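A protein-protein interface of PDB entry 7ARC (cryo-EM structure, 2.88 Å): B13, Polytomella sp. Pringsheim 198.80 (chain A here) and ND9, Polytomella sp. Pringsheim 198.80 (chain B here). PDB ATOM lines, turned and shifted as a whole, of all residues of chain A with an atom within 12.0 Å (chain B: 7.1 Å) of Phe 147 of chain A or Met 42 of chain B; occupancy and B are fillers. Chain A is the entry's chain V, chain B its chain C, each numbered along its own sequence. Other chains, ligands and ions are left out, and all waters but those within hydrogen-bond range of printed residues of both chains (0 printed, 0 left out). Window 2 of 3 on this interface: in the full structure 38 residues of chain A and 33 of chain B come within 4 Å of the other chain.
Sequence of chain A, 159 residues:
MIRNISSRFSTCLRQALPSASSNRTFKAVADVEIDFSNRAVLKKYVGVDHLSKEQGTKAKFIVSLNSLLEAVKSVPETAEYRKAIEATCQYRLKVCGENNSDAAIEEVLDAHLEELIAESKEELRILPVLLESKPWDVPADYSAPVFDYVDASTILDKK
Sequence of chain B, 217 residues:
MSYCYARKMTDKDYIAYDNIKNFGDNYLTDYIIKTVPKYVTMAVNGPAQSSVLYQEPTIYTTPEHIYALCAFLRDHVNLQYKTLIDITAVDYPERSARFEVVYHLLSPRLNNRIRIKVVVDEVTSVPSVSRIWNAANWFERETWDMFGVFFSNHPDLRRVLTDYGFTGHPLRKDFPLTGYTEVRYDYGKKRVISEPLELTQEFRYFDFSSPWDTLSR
OH of Tyr 142 of chain A lies within hydrogen-bond range of O of Val 40 of chain B (2.8 Å).
The backbone NH (N) of Ala 43 of chain B sits at hydrogen-bond distance from the backbone carbonyl oxygen (O) of Pro 145 of chain A (3.0 Å).
N of Phe 147 of chain A sits at hydrogen-bond distance from O of Ala 43 of chain B (2.9 Å).
The backbone NH (N) of Asn 45 of chain B sits at hydrogen-bond distance from the backbone carbonyl oxygen (O) of Phe 147 of chain A, at 2.5 Å.
The side-chain amide nitrogen (ND2) of Asn 45 of chain B is in hydrogen-bond range of the side-chain carboxylate (OD1) of Asp 148 of chain A.
The backbone NH (N) of Tyr 149 of chain A is in hydrogen-bond range of the backbone carbonyl oxygen (O) of Asn 45 of chain B (3.0 Å).
The side-chain amide oxygen of Asn 45 of chain B lies within hydrogen-bond range of the side-chain hydroxyl of Thr 29 of chain B (3.2 Å).
The side-chain hydroxyl (OG1) of Thr 41 of chain B sits at hydrogen-bond distance from the backbone carbonyl oxygen (O) of Tyr 60 of chain B (3.0 Å).
N of Tyr 60 of chain B is in hydrogen-bond range of O of Met 42 of chain B (2.9 Å).
The backbone carbonyl oxygen of Val 44 of chain B lies within hydrogen-bond range of the backbone NH of Thr 58 of chain B (2.7 Å).
Among the printed residues, merely in contact across the chains: Ala 144 of chain A with Ile 33 of chain B (3.9 Å), Ala 144 of chain A with Thr 41 of chain B (3.9 Å), Pro 145 of chain A with Thr 41 of chain B (3.4 Å), Pro 145 of chain A with Met 42 of chain B (3.4 Å), Val 146 of chain A with Ile 33 of chain B (3.6 Å), Val 146 of chain A with Ala 43 of chain B (3.2 Å), Val 146 of chain A with Asn 45 of chain B (3.9 Å), Phe 147 of chain A with Met 42 of chain B (3.6 Å), Phe 147 of chain A with Val 44 of chain B (3.4 Å) and Tyr 149 of chain A with Gly 46 of chain B (3.5 Å).
Of the printed residues of chain B, Ala 144 of chain A touches Ile 33 (3.9 Å) and Thr 41 (3.9 Å).
Of the printed residues of chain B, Pro 145 of chain A touches Thr 41, Met 42 and Ala 43.
Of chain B, only Met 42 (3.6 Å), Ala 43 (2.9 Å), Val 44 (3.4 Å) and Asn 45 (2.5 Å) come within 4 Å of Phe 147 of chain A.
Of the printed residues of chain B, Asp 148 of chain A touches Asn 45 (2.9 Å).
Printed residues of chain A within 4 Å of Ile 33 of chain B: Ala 144 and Val 146.
Of chain A, only Ala 144 (3.9 Å) and Pro 145 (3.4 Å) come within 4 Å of Thr 41 of chain B.
Of chain A, only Pro 145 (3.4 Å) and Phe 147 (3.6 Å) come within 4 Å of Met 42 of chain B.
Of chain A, only Pro 145 (3.0 Å), Val 146 (3.2 Å) and Phe 147 (2.9 Å) come within 4 Å of Ala 43 of chain B.
Printed residues of chain A within 4 Å of Val 44 of chain B: Phe 147 (3.4 Å).
Gly 46 of chain B touches just one residue of chain A: Tyr 149 (3.5 Å).
No residue of chain A comes within 4 Å of Ile 59 of chain B.
No residue of chain A comes within 4 Å of Thr 61 of chain B.
Printed residues of chain A that touch a printed residue of chain B: Tyr 142, Ala 144, Pro 145, Val 146, Phe 147, Asp 148 and Tyr 149.
Hydrophobic or aromatic side chains of chain A within 4 Å of the printed part of chain B: Tyr 142, Ala 144, Pro 145, Val 146, Phe 147 and Tyr 149.
Of the 14 printed residues of chain B, 8 touch a printed residue of chain A.
Hydrophobic or aromatic side chains of chain B within 4 Å of the printed part of chain A: Ile 33, Val 40, Met 42, Ala 43 and Val 44.
Among the printed residues, 16 pairs touch across the chains.
Among the printed residues, no Asp or Glu carboxylate lies within 4 Å of a Lys or Arg side-chain nitrogen of the other chain.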
ATOM      1  N   VAL A 138     -13.583 -28.186   5.298  1.00  0.00           N
ATOM      2  CA  VAL A 138     -12.989 -27.953   3.982  1.00  0.00           C
ATOM      3  C   VAL A 138     -11.939 -26.861   4.093  1.00  0.00           C
ATOM      4  O   VAL A 138     -11.974 -26.030   5.011  1.00  0.00           O
ATOM      5  CB  VAL A 138     -14.046 -27.567   2.926  1.00  0.00           C
ATOM      6  CG1 VAL A 138     -15.041 -28.692   2.727  1.00  0.00           C
ATOM      7  CG2 VAL A 138     -14.766 -26.297   3.338  1.00  0.00           C
ATOM      8  N   TYR A 142     -11.881 -23.556  -0.760  1.00  0.00           N
ATOM      9  CA  TYR A 142     -12.809 -24.465  -1.419  1.00  0.00           C
ATOM     10  C   TYR A 142     -13.734 -23.700  -2.355  1.00  0.00           C
ATOM     11  O   TYR A 142     -14.272 -22.649  -1.995  1.00  0.00           O
ATOM     12  CB  TYR A 142     -13.617 -25.231  -0.370  1.00  0.00           C
ATOM     13  CG  TYR A 142     -14.779 -26.022  -0.927  1.00  0.00           C
ATOM     14  CD1 TYR A 142     -16.061 -25.486  -0.951  1.00  0.00           C
ATOM     15  CD2 TYR A 142     -14.597 -27.303  -1.426  1.00  0.00           C
ATOM     16  CE1 TYR A 142     -17.123 -26.202  -1.457  1.00  0.00           C
ATOM     17  CE2 TYR A 142     -15.653 -28.027  -1.935  1.00  0.00           C
ATOM     18  CZ  TYR A 142     -16.915 -27.471  -1.948  1.00  0.00           C
ATOM     19  OH  TYR A 142     -17.975 -28.186  -2.454  1.00  0.00           O
ATOM     20  N   SER A 143     -13.914 -24.229  -3.563  1.00  0.00           N
ATOM     21  CA  SER A 143     -14.723 -23.579  -4.588  1.00  0.00           C
ATOM     22  C   SER A 143     -15.452 -24.644  -5.390  1.00  0.00           C
ATOM     23  O   SER A 143     -14.816 -25.506  -6.003  1.00  0.00           O
ATOM     24  CB  SER A 143     -13.859 -22.714  -5.510  1.00  0.00           C
ATOM     25  OG  SER A 143     -14.640 -22.111  -6.525  1.00  0.00           O
ATOM     26  N   ALA A 144     -16.781 -24.581  -5.386  1.00  0.00           N
ATOM     27  CA  ALA A 144     -17.611 -25.532  -6.116  1.00  0.00           C
ATOM     28  C   ALA A 144     -18.181 -24.858  -7.353  1.00  0.00           C
ATOM     29  O   ALA A 144     -19.029 -23.961  -7.226  1.00  0.00           O
ATOM     30  CB  ALA A 144     -18.738 -26.063  -5.230  1.00  0.00           C
ATOM     31  N   PRO A 145     -17.753 -25.235  -8.557  1.00  0.00           N
ATOM     32  CA  PRO A 145     -18.274 -24.584  -9.765  1.00  0.00           C
ATOM     33  C   PRO A 145     -19.739 -24.931  -9.983  1.00  0.00           C
ATOM     34  O   PRO A 145     -20.139 -26.090  -9.872  1.00  0.00           O
ATOM     35  CB  PRO A 145     -17.394 -25.158 -10.881  1.00  0.00           C
ATOM     36  CG  PRO A 145     -16.153 -25.603 -10.190  1.00  0.00           C
ATOM     37  CD  PRO A 145     -16.604 -26.105  -8.855  1.00  0.00           C
ATOM     38  N   VAL A 146     -20.538 -23.914 -10.293  1.00  0.00           N
ATOM     39  CA  VAL A 146     -21.973 -24.070 -10.489  1.00  0.00           C
ATOM     40  C   VAL A 146     -22.322 -23.578 -11.885  1.00  0.00           C
ATOM     41  O   VAL A 146     -21.997 -22.444 -12.250  1.00  0.00           O
ATOM     42  CB  VAL A 146     -22.780 -23.314  -9.421  1.00  0.00           C
ATOM     43  CG1 VAL A 146     -24.193 -23.069  -9.907  1.00  0.00           C
ATOM     44  CG2 VAL A 146     -22.799 -24.105  -8.138  1.00  0.00           C
ATOM     45  N   PHE A 147     -22.985 -24.433 -12.655  1.00  0.00           N
ATOM     46  CA  PHE A 147     -23.421 -24.124 -14.008  1.00  0.00           C
ATOM     47  C   PHE A 147     -24.929 -23.931 -14.014  1.00  0.00           C
ATOM     48  O   PHE A 147     -25.668 -24.770 -13.489  1.00  0.00           O
ATOM     49  CB  PHE A 147     -23.017 -25.239 -14.971  1.00  0.00           C
ATOM     50  CG  PHE A 147     -21.536 -25.331 -15.193  1.00  0.00           C
ATOM     51  CD1 PHE A 147     -20.727 -25.985 -14.279  1.00  0.00           C
ATOM     52  CD2 PHE A 147     -20.948 -24.756 -16.305  1.00  0.00           C
ATOM     53  CE1 PHE A 147     -19.366 -26.069 -14.473  1.00  0.00           C
ATOM     54  CE2 PHE A 147     -19.585 -24.837 -16.504  1.00  0.00           C
ATOM     55  CZ  PHE A 147     -18.793 -25.495 -15.586  1.00  0.00           C
ATOM     56  N   ASP A 148     -25.384 -22.830 -14.603  1.00  0.00           N
ATOM     57  CA  ASP A 148     -26.789 -22.452 -14.587  1.00  0.00           C
ATOM     58  C   ASP A 148     -27.312 -22.360 -16.012  1.00  0.00           C
ATOM     59  O   ASP A 148     -26.591 -21.940 -16.922  1.00  0.00           O
ATOM     60  CB  ASP A 148     -26.992 -21.118 -13.870  1.00  0.00           C
ATOM     61  CG  ASP A 148     -26.723 -21.206 -12.383  1.00  0.00           C
ATOM     62  OD1 ASP A 148     -26.921 -22.293 -11.802  1.00  0.00           O
ATOM     63  OD2 ASP A 148     -26.310 -20.187 -11.794  1.00  0.00           O
ATOM     64  N   TYR A 149     -28.568 -22.753 -16.195  1.00  0.00           N
ATOM     65  CA  TYR A 149     -29.204 -22.817 -17.504  1.00  0.00           C
ATOM     66  C   TYR A 149     -30.031 -21.563 -17.752  1.00  0.00           C
ATOM     67  O   TYR A 149     -30.841 -21.170 -16.907  1.00  0.00           O
ATOM     68  CB  TYR A 149     -30.087 -24.060 -17.596  1.00  0.00           C
ATOM     69  CG  TYR A 149     -31.041 -24.093 -18.766  1.00  0.00           C
ATOM     70  CD1 TYR A 149     -30.595 -24.405 -20.043  1.00  0.00           C
ATOM     71  CD2 TYR A 149     -32.391 -23.831 -18.590  1.00  0.00           C
ATOM     72  CE1 TYR A 149     -31.466 -24.446 -21.111  1.00  0.00           C
ATOM     73  CE2 TYR A 149     -33.268 -23.867 -19.652  1.00  0.00           C
ATOM     74  CZ  TYR A 149     -32.801 -24.175 -20.910  1.00  0.00           C
ATOM     75  OH  TYR A 149     -33.677 -24.212 -21.971  1.00  0.00           O
ATOM     76  N   VAL A 150     -29.822 -20.940 -18.908  1.00  0.00           N
ATOM     77  CA  VAL A 150     -30.555 -19.747 -19.320  1.00  0.00           C
ATOM     78  C   VAL A 150     -31.495 -20.141 -20.450  1.00  0.00           C
ATOM     79  O   VAL A 150     -31.058 -20.675 -21.476  1.00  0.00           O
ATOM     80  CB  VAL A 150     -29.609 -18.620 -19.760  1.00  0.00           C
ATOM     81  CG1 VAL A 150     -30.377 -17.318 -19.905  1.00  0.00           C
ATOM     82  CG2 VAL A 150     -28.471 -18.466 -18.765  1.00  0.00           C
ATOM     83  N   ASP A 151     -32.784 -19.873 -20.265  1.00  0.00           N
ATOM     84  CA  ASP A 151     -33.791 -20.265 -21.241  1.00  0.00           C
ATOM     85  C   ASP A 151     -33.862 -19.262 -22.386  1.00  0.00           C
ATOM     86  O   ASP A 151     -33.741 -18.050 -22.181  1.00  0.00           O
ATOM     87  CB  ASP A 151     -35.160 -20.384 -20.574  1.00  0.00           C
ATOM     88  CG  ASP A 151     -36.092 -21.317 -21.318  1.00  0.00           C
ATOM     89  OD1 ASP A 151     -36.453 -21.001 -22.471  1.00  0.00           O
ATOM     90  OD2 ASP A 151     -36.468 -22.363 -20.749  1.00  0.00           O
ATOM     91  N   THR B  29     -29.322 -25.476  -4.472  1.00  0.00           N
ATOM     92  CA  THR B  29     -27.937 -25.821  -4.770  1.00  0.00           C
ATOM     93  C   THR B  29     -26.972 -25.117  -3.827  1.00  0.00           C
ATOM     94  O   THR B  29     -26.020 -25.732  -3.331  1.00  0.00           O
ATOM     95  CB  THR B  29     -27.628 -25.463  -6.221  1.00  0.00           C
ATOM     96  OG1 THR B  29     -28.516 -26.175  -7.089  1.00  0.00           O
ATOM     97  CG2 THR B  29     -26.215 -25.825  -6.564  1.00  0.00           C
ATOM     98  N   ILE B  33     -24.409 -27.012  -1.225  1.00  0.00           N
ATOM     99  CA  ILE B  33     -22.966 -26.781  -1.270  1.00  0.00           C
ATOM    100  C   ILE B  33     -22.466 -26.240   0.063  1.00  0.00           C
ATOM    101  O   ILE B  33     -21.441 -26.687   0.588  1.00  0.00           O
ATOM    102  CB  ILE B  33     -22.600 -25.845  -2.434  1.00  0.00           C
ATOM    103  CG1 ILE B  33     -22.734 -26.584  -3.764  1.00  0.00           C
ATOM    104  CG2 ILE B  33     -21.192 -25.311  -2.268  1.00  0.00           C
ATOM    105  CD1 ILE B  33     -23.064 -25.690  -4.917  1.00  0.00           C
ATOM    106  N   TYR B  39     -18.655 -33.139   0.225  1.00  0.00           N
ATOM    107  CA  TYR B  39     -19.239 -34.126  -0.679  1.00  0.00           C
ATOM    108  C   TYR B  39     -19.337 -33.595  -2.105  1.00  0.00           C
ATOM    109  O   TYR B  39     -19.101 -34.336  -3.064  1.00  0.00           O
ATOM    110  CB  TYR B  39     -20.613 -34.559  -0.170  1.00  0.00           C
ATOM    111  CG  TYR B  39     -20.620 -35.091   1.246  1.00  0.00           C
ATOM    112  CD1 TYR B  39     -19.465 -35.589   1.831  1.00  0.00           C
ATOM    113  CD2 TYR B  39     -21.787 -35.103   1.993  1.00  0.00           C
ATOM    114  CE1 TYR B  39     -19.472 -36.078   3.116  1.00  0.00           C
ATOM    115  CE2 TYR B  39     -21.803 -35.590   3.281  1.00  0.00           C
ATOM    116  CZ  TYR B  39     -20.643 -36.076   3.837  1.00  0.00           C
ATOM    117  OH  TYR B  39     -20.654 -36.564   5.121  1.00  0.00           O
ATOM    118  N   VAL B  40     -19.679 -32.323  -2.263  1.00  0.00           N
ATOM    119  CA  VAL B  40     -19.974 -31.766  -3.577  1.00  0.00           C
ATOM    120  C   VAL B  40     -18.680 -31.333  -4.251  1.00  0.00           C
ATOM    121  O   VAL B  40     -17.823 -30.696  -3.629  1.00  0.00           O
ATOM    122  CB  VAL B  40     -20.954 -30.589  -3.453  1.00  0.00           C
ATOM    123  CG1 VAL B  40     -21.186 -29.941  -4.805  1.00  0.00           C
ATOM    124  CG2 VAL B  40     -22.258 -31.052  -2.835  1.00  0.00           C
ATOM    125  N   THR B  41     -18.533 -31.679  -5.528  1.00  0.00           N
ATOM    126  CA  THR B  41     -17.434 -31.201  -6.359  1.00  0.00           C
ATOM    127  C   THR B  41     -17.863 -30.154  -7.375  1.00  0.00           C
ATOM    128  O   THR B  41     -17.159 -29.162  -7.564  1.00  0.00           O
ATOM    129  CB  THR B  41     -16.766 -32.369  -7.091  1.00  0.00           C
ATOM    130  OG1 THR B  41     -17.583 -32.773  -8.196  1.00  0.00           O
ATOM    131  CG2 THR B  41     -16.574 -33.544  -6.153  1.00  0.00           C
ATOM    132  N   MET B  42     -19.000 -30.353  -8.036  1.00  0.00           N
ATOM    133  CA  MET B  42     -19.586 -29.345  -8.905  1.00  0.00           C
ATOM    134  C   MET B  42     -21.092 -29.549  -8.940  1.00  0.00           C
ATOM    135  O   MET B  42     -21.601 -30.616  -8.594  1.00  0.00           O
ATOM    136  CB  MET B  42     -19.017 -29.395 -10.328  1.00  0.00           C
ATOM    137  CG  MET B  42     -19.341 -30.670 -11.076  1.00  0.00           C
ATOM    138  SD  MET B  42     -18.685 -30.711 -12.752  1.00  0.00           S
ATOM    139  CE  MET B  42     -19.767 -29.535 -13.557  1.00  0.00           C
ATOM    140  N   ALA B  43     -21.801 -28.505  -9.353  1.00  0.00           N
ATOM    141  CA  ALA B  43     -23.254 -28.518  -9.424  1.00  0.00           C
ATOM    142  C   ALA B  43     -23.704 -27.924 -10.748  1.00  0.00           C
ATOM    143  O   ALA B  43     -23.087 -26.987 -11.256  1.00  0.00           O
ATOM    144  CB  ALA B  43     -23.866 -27.742  -8.267  1.00  0.00           C
ATOM    145  N   VAL B  44     -24.777 -28.477 -11.308  1.00  0.00           N
ATOM    146  CA  VAL B  44     -25.370 -27.982 -12.544  1.00  0.00           C
ATOM    147  C   VAL B  44     -26.855 -27.737 -12.321  1.00  0.00           C
ATOM    148  O   VAL B  44     -27.574 -28.631 -11.863  1.00  0.00           O
ATOM    149  CB  VAL B  44     -25.155 -28.964 -13.712  1.00  0.00           C
ATOM    150  CG1 VAL B  44     -25.849 -28.463 -14.961  1.00  0.00           C
ATOM    151  CG2 VAL B  44     -23.677 -29.167 -13.971  1.00  0.00           C
ATOM    152  N   ASN B  45     -27.308 -26.526 -12.635  1.00  0.00           N
ATOM    153  CA  ASN B  45     -28.726 -26.192 -12.706  1.00  0.00           C
ATOM    154  C   ASN B  45     -29.165 -26.190 -14.165  1.00  0.00           C
ATOM    155  O   ASN B  45     -28.561 -25.500 -14.993  1.00  0.00           O
ATOM    156  CB  ASN B  45     -28.995 -24.825 -12.078  1.00  0.00           C
ATOM    157  CG  ASN B  45     -28.974 -24.864 -10.568  1.00  0.00           C
ATOM    158  OD1 ASN B  45     -29.874 -25.413  -9.937  1.00  0.00           O
ATOM    159  ND2 ASN B  45     -27.943 -24.274  -9.978  1.00  0.00           N
ATOM    160  N   GLY B  46     -30.212 -26.949 -14.480  1.00  0.00           N
ATOM    161  CA  GLY B  46     -30.631 -27.096 -15.856  1.00  0.00           C
ATOM    162  C   GLY B  46     -32.124 -27.267 -16.057  1.00  0.00           C
ATOM    163  O   GLY B  46     -32.932 -27.002 -15.161  1.00  0.00           O
ATOM    164  N   THR B  58     -28.358 -30.643 -10.217  1.00  0.00           N
ATOM    165  CA  THR B  58     -27.595 -31.862 -10.434  1.00  0.00           C
ATOM    166  C   THR B  58     -26.273 -31.689  -9.708  1.00  0.00           C
ATOM    167  O   THR B  58     -25.578 -30.689  -9.906  1.00  0.00           O
ATOM    168  CB  THR B  58     -27.351 -32.124 -11.924  1.00  0.00           C
ATOM    169  OG1 THR B  58     -28.603 -32.268 -12.602  1.00  0.00           O
ATOM    170  CG2 THR B  58     -26.531 -33.387 -12.117  1.00  0.00           C
ATOM    171  N   ILE B  59     -25.933 -32.665  -8.876  1.00  0.00           N
ATOM    172  CA  ILE B  59     -24.746 -32.622  -8.035  1.00  0.00           C
ATOM    173  C   ILE B  59     -23.806 -33.735  -8.464  1.00  0.00           C
ATOM    174  O   ILE B  59     -24.227 -34.885  -8.620  1.00  0.00           O
ATOM    175  CB  ILE B  59     -25.110 -32.777  -6.547  1.00  0.00           C
ATOM    176  CG1 ILE B  59     -26.065 -31.669  -6.101  1.00  0.00           C
ATOM    177  CG2 ILE B  59     -23.863 -32.770  -5.688  1.00  0.00           C
ATOM    178  CD1 ILE B  59     -25.500 -30.284  -6.230  1.00  0.00           C
ATOM    179  N   TYR B  60     -22.539 -33.387  -8.662  1.00  0.00           N
ATOM    180  CA  TYR B  60     -21.491 -34.354  -8.951  1.00  0.00           C
ATOM    181  C   TYR B  60     -20.717 -34.598  -7.666  1.00  0.00           C
ATOM    182  O   TYR B  60     -20.220 -33.654  -7.048  1.00  0.00           O
ATOM    183  CB  TYR B  60     -20.552 -33.854 -10.046  1.00  0.00           C
ATOM    184  CG  TYR B  60     -21.170 -33.742 -11.417  1.00  0.00           C
ATOM    185  CD1 TYR B  60     -22.093 -32.751 -11.706  1.00  0.00           C
ATOM    186  CD2 TYR B  60     -20.816 -34.621 -12.427  1.00  0.00           C
ATOM    187  CE1 TYR B  60     -22.650 -32.644 -12.960  1.00  0.00           C
ATOM    188  CE2 TYR B  60     -21.368 -34.521 -13.683  1.00  0.00           C
ATOM    189  CZ  TYR B  60     -22.285 -33.532 -13.944  1.00  0.00           C
ATOM    190  OH  TYR B  60     -22.839 -33.430 -15.197  1.00  0.00           O
ATOM    191  N   THR B  61     -20.621 -35.861  -7.267  1.00  0.00           N
ATOM    192  CA  THR B  61     -19.879 -36.240  -6.079  1.00  0.00           C
ATOM    193  C   THR B  61     -19.025 -37.457  -6.399  1.00  0.00           C
ATOM    194  O   THR B  61     -19.218 -38.128  -7.414  1.00  0.00           O
ATOM    195  CB  THR B  61     -20.814 -36.526  -4.896  1.00  0.00           C
ATOM    196  OG1 THR B  61     -20.043 -36.750  -3.711  1.00  0.00           O
ATOM    197  CG2 THR B  61     -21.664 -37.744  -5.174  1.00  0.00           C
